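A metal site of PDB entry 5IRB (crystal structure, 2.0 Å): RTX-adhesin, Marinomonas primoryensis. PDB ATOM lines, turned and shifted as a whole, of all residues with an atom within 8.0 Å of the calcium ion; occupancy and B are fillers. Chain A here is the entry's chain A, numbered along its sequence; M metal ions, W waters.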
ATOM      1  N   VAL A  49       9.684 -22.658  22.621  1.00  0.00           N
ATOM      2  CA  VAL A  49      10.785 -23.616  22.596  1.00  0.00           C
ATOM      3  C   VAL A  49      10.379 -24.871  23.336  1.00  0.00           C
ATOM      4  O   VAL A  49       9.896 -24.810  24.458  1.00  0.00           O
ATOM      5  CB  VAL A  49      12.095 -23.042  23.195  1.00  0.00           C
ATOM      6  CG1 VAL A  49      13.200 -24.111  23.175  1.00  0.00           C
ATOM      7  CG2 VAL A  49      12.523 -21.782  22.431  1.00  0.00           C
ATOM      8  N   ILE A  50      10.591 -26.020  22.698  1.00  0.00           N
ATOM      9  CA  ILE A  50      10.200 -27.302  23.259  1.00  0.00           C
ATOM     10  C   ILE A  50      11.222 -28.320  22.830  1.00  0.00           C
ATOM     11  O   ILE A  50      11.482 -28.502  21.632  1.00  0.00           O
ATOM     12  CB  ILE A  50       8.800 -27.758  22.772  1.00  0.00           C
ATOM     13  CG1 ILE A  50       7.734 -26.693  23.025  1.00  0.00           C
ATOM     14  CG2 ILE A  50       8.412 -29.071  23.432  1.00  0.00           C
ATOM     15  CD1 ILE A  50       6.591 -26.741  22.028  1.00  0.00           C
ATOM     16  N   ASN A  51      11.805 -28.980  23.826  1.00  0.00           N
ATOM     17  CA  ASN A  51      12.819 -30.020  23.589  1.00  0.00           C
ATOM     18  C   ASN A  51      13.971 -29.441  22.746  1.00  0.00           C
ATOM     19  O   ASN A  51      14.489 -30.101  21.849  1.00  0.00           O
ATOM     20  CB  ASN A  51      12.164 -31.241  22.916  1.00  0.00           C
ATOM     21  CG  ASN A  51      13.121 -32.443  22.778  1.00  0.00           C
ATOM     22  OD1 ASN A  51      13.930 -32.705  23.656  1.00  0.00           O
ATOM     23  ND2 ASN A  51      13.011 -33.167  21.674  1.00  0.00           N
ATOM     24  N   GLY A  52      14.342 -28.186  23.045  1.00  0.00           N
ATOM     25  CA  GLY A  52      15.318 -27.449  22.254  1.00  0.00           C
ATOM     26  C   GLY A  52      14.909 -27.020  20.850  1.00  0.00           C
ATOM     27  O   GLY A  52      15.714 -26.468  20.078  1.00  0.00           O
ATOM     28  N   ASP A  73       8.446 -33.758  20.459  1.00  0.00           N
ATOM     29  CA  ASP A  73       9.156 -32.727  21.209  1.00  0.00           C
ATOM     30  C   ASP A  73       8.487 -32.472  22.551  1.00  0.00           C
ATOM     31  O   ASP A  73       9.182 -32.298  23.551  1.00  0.00           O
ATOM     32  CB  ASP A  73       9.251 -31.450  20.378  1.00  0.00           C
ATOM     33  CG  ASP A  73      10.245 -31.580  19.248  1.00  0.00           C
ATOM     34  OD1 ASP A  73      11.222 -32.349  19.427  1.00  0.00           O
ATOM     35  OD2 ASP A  73      10.062 -30.943  18.193  1.00  0.00           O
ATOM     36  N   LEU A  74       7.167 -32.466  22.583  1.00  0.00           N
ATOM     37  CA  LEU A  74       6.469 -32.326  23.859  1.00  0.00           C
ATOM     38  C   LEU A  74       6.773 -33.537  24.770  1.00  0.00           C
ATOM     39  O   LEU A  74       7.120 -33.389  25.940  1.00  0.00           O
ATOM     40  CB  LEU A  74       4.957 -32.183  23.638  1.00  0.00           C
ATOM     41  CG  LEU A  74       4.426 -30.868  23.050  1.00  0.00           C
ATOM     42  CD1 LEU A  74       2.997 -31.022  22.539  1.00  0.00           C
ATOM     43  CD2 LEU A  74       4.509 -29.783  24.117  1.00  0.00           C
ATOM     44  N   ALA A  76       9.329 -35.558  24.704  1.00  0.00           N
ATOM     45  CA  ALA A  76      10.747 -35.567  25.066  1.00  0.00           C
ATOM     46  C   ALA A  76      11.184 -34.390  25.940  1.00  0.00           C
ATOM     47  O   ALA A  76      12.264 -34.450  26.550  1.00  0.00           O
ATOM     48  CB  ALA A  76      11.615 -35.616  23.814  1.00  0.00           C
ATOM     49  N   ASP A  77      10.397 -33.316  25.982  1.00  0.00           N
ATOM     50  CA  ASP A  77      10.847 -32.089  26.649  1.00  0.00           C
ATOM     51  C   ASP A  77      11.174 -32.369  28.118  1.00  0.00           C
ATOM     52  O   ASP A  77      10.297 -32.732  28.905  1.00  0.00           O
ATOM     53  CB  ASP A  77       9.769 -30.988  26.529  1.00  0.00           C
ATOM     54  CG  ASP A  77      10.173 -29.685  27.215  1.00  0.00           C
ATOM     55  OD1 ASP A  77      10.903 -28.854  26.594  1.00  0.00           O
ATOM     56  OD2 ASP A  77       9.756 -29.482  28.392  1.00  0.00           O
ATOM     57  N   SER A  78      12.443 -32.163  28.465  1.00  0.00           N
ATOM     58  CA  SER A  78      12.976 -32.641  29.746  1.00  0.00           C
ATOM     59  C   SER A  78      12.185 -32.163  30.961  1.00  0.00           C
ATOM     60  O   SER A  78      11.904 -32.972  31.851  1.00  0.00           O
ATOM     61  CB  SER A  78      14.438 -32.244  29.904  1.00  0.00           C
ATOM     62  OG  SER A  78      14.659 -30.939  29.427  1.00  0.00           O
ATOM     63  N   ASP A  79      11.824 -30.881  31.030  1.00  0.00           N
ATOM     64  CA  ASP A  79      11.126 -30.438  32.239  1.00  0.00           C
ATOM     65  C   ASP A  79       9.609 -30.372  32.089  1.00  0.00           C
ATOM     66  O   ASP A  79       8.937 -29.911  32.992  1.00  0.00           O
ATOM     67  CB  ASP A  79      11.667 -29.092  32.709  1.00  0.00           C
ATOM     68  CG  ASP A  79      11.502 -27.992  31.673  1.00  0.00           C
ATOM     69  OD1 ASP A  79      11.050 -28.268  30.561  1.00  0.00           O
ATOM     70  OD2 ASP A  79      11.838 -26.834  31.989  1.00  0.00           O
ATOM     71  N   ARG A  80       9.086 -30.862  30.969  1.00  0.00           N
ATOM     72  CA  ARG A  80       7.646 -30.793  30.696  1.00  0.00           C
ATOM     73  C   ARG A  80       7.128 -29.347  30.847  1.00  0.00           C
ATOM     74  O   ARG A  80       6.074 -29.103  31.432  1.00  0.00           O
ATOM     75  CB  ARG A  80       6.854 -31.758  31.598  1.00  0.00           C
ATOM     76  CG  ARG A  80       6.890 -33.240  31.154  1.00  0.00           C
ATOM     77  CD  ARG A  80       8.171 -33.962  31.554  1.00  0.00           C
ATOM     78  NE  ARG A  80       8.078 -35.406  31.323  1.00  0.00           N
ATOM     79  CZ  ARG A  80       8.342 -36.018  30.175  1.00  0.00           C
ATOM     80  NH1 ARG A  80       8.739 -35.318  29.116  1.00  0.00           N
ATOM     81  NH2 ARG A  80       8.231 -37.334  30.065  1.00  0.00           N
ATOM     82  N   ILE A  81       7.920 -28.403  30.342  1.00  0.00           N
ATOM     83  CA  ILE A  81       7.529 -26.987  30.312  1.00  0.00           C
ATOM     84  C   ILE A  81       7.771 -26.421  28.930  1.00  0.00           C
ATOM     85  O   ILE A  81       8.866 -26.575  28.389  1.00  0.00           O
ATOM     86  CB  ILE A  81       8.291 -26.126  31.337  1.00  0.00           C
ATOM     87  CG1 ILE A  81       8.023 -26.581  32.762  1.00  0.00           C
ATOM     88  CG2 ILE A  81       7.920 -24.651  31.202  1.00  0.00           C
ATOM     89  CD1 ILE A  81       9.066 -26.068  33.723  1.00  0.00           C
ATOM     90  N   VAL A  82       6.740 -25.799  28.376  1.00  0.00           N
ATOM     91  CA  VAL A  82       6.861 -25.021  27.161  1.00  0.00           C
ATOM     92  C   VAL A  82       7.362 -23.609  27.542  1.00  0.00           C
ATOM     93  O   VAL A  82       6.711 -22.945  28.343  1.00  0.00           O
ATOM     94  CB  VAL A  82       5.518 -24.918  26.420  1.00  0.00           C
ATOM     95  CG1 VAL A  82       5.662 -24.011  25.188  1.00  0.00           C
ATOM     96  CG2 VAL A  82       5.001 -26.301  26.026  1.00  0.00           C
ATOM     97  N   ASP A  83       8.492 -23.175  26.989  1.00  0.00           N
ATOM     98  CA  ASP A  83       8.935 -21.775  27.155  1.00  0.00           C
ATOM     99  C   ASP A  83       8.450 -20.943  25.964  1.00  0.00           C
ATOM    100  O   ASP A  83       8.637 -21.329  24.811  1.00  0.00           O
ATOM    101  CB  ASP A  83      10.457 -21.670  27.293  1.00  0.00           C
ATOM    102  CG  ASP A  83      11.024 -22.537  28.428  1.00  0.00           C
ATOM    103  OD1 ASP A  83      10.506 -22.479  29.580  1.00  0.00           O
ATOM    104  OD2 ASP A  83      12.019 -23.259  28.191  1.00  0.00           O
ATOM    105  N   GLU A 102       4.408 -22.792  30.191  1.00  0.00           N
ATOM    106  CA  GLU A 102       3.270 -23.683  30.357  1.00  0.00           C
ATOM    107  C   GLU A 102       3.792 -25.088  30.658  1.00  0.00           C
ATOM    108  O   GLU A 102       4.494 -25.692  29.857  1.00  0.00           O
ATOM    109  CB  GLU A 102       2.410 -23.693  29.089  1.00  0.00           C
ATOM    110  CG  GLU A 102       1.084 -24.449  29.240  1.00  0.00           C
ATOM    111  CD  GLU A 102       0.190 -23.832  30.276  1.00  0.00           C
ATOM    112  OE1 GLU A 102       0.361 -22.624  30.561  1.00  0.00           O
ATOM    113  OE2 GLU A 102      -0.678 -24.542  30.819  1.00  0.00           O
ATOM    114  N   PHE A 104       3.059 -29.145  31.582  1.00  0.00           N
ATOM    115  CA  PHE A 104       2.111 -30.146  31.141  1.00  0.00           C
ATOM    116  C   PHE A 104       2.559 -31.490  31.675  1.00  0.00           C
ATOM    117  O   PHE A 104       3.657 -31.614  32.230  1.00  0.00           O
ATOM    118  CB  PHE A 104       1.964 -30.147  29.626  1.00  0.00           C
ATOM    119  CG  PHE A 104       3.237 -30.396  28.897  1.00  0.00           C
ATOM    120  CD1 PHE A 104       4.141 -29.357  28.669  1.00  0.00           C
ATOM    121  CD2 PHE A 104       3.554 -31.656  28.432  1.00  0.00           C
ATOM    122  CE1 PHE A 104       5.324 -29.578  28.015  1.00  0.00           C
ATOM    123  CE2 PHE A 104       4.741 -31.888  27.772  1.00  0.00           C
ATOM    124  CZ  PHE A 104       5.628 -30.846  27.558  1.00  0.00           C
HETATM  125 CA    CA M   1      11.109 -27.304  28.402  1.00  0.00          CA
HETATM  126  O   HOH W   1      11.628 -25.738  26.457  1.00  0.00           O
HETATM  127  O   HOH W   2      11.969 -25.413  29.729  1.00  0.00           O
HETATM  128  O   HOH W   3      13.465 -28.241  28.265  1.00  0.00           O
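Water W1 bridges O of Val 49 (2.8 Å) and OD2 of Asp 83 (3.1 Å).
Water W2 bridges the side-chain carboxylate of Asp 83 (2.6 Å) and the side-chain carboxylate of Asp 79 (2.7 Å).
The calcium ion is bound by O of Ile 81 (2.4 Å), OD1 of Asp 79 (2.4 Å), OD1 of Asp 77 (2.4 Å), water W2 (2.5 Å), water W3 (2.5 Å), water W1 (2.6 Å) and OD2 of Asp 77 (2.6 Å).
Three residues have an atom within 4 Å of the calcium ion: Asp 77, Asp 79 and Ile 81.
The side-chain carboxylate (OD1) of Asp 77 sits close to the backbone NH (N) of Asn 51 (2.9 Å).
The backbone carbonyl oxygen of Asp 77 lies within hydrogen-bond range of the guanidinium group of Arg 80 (3.0 Å).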
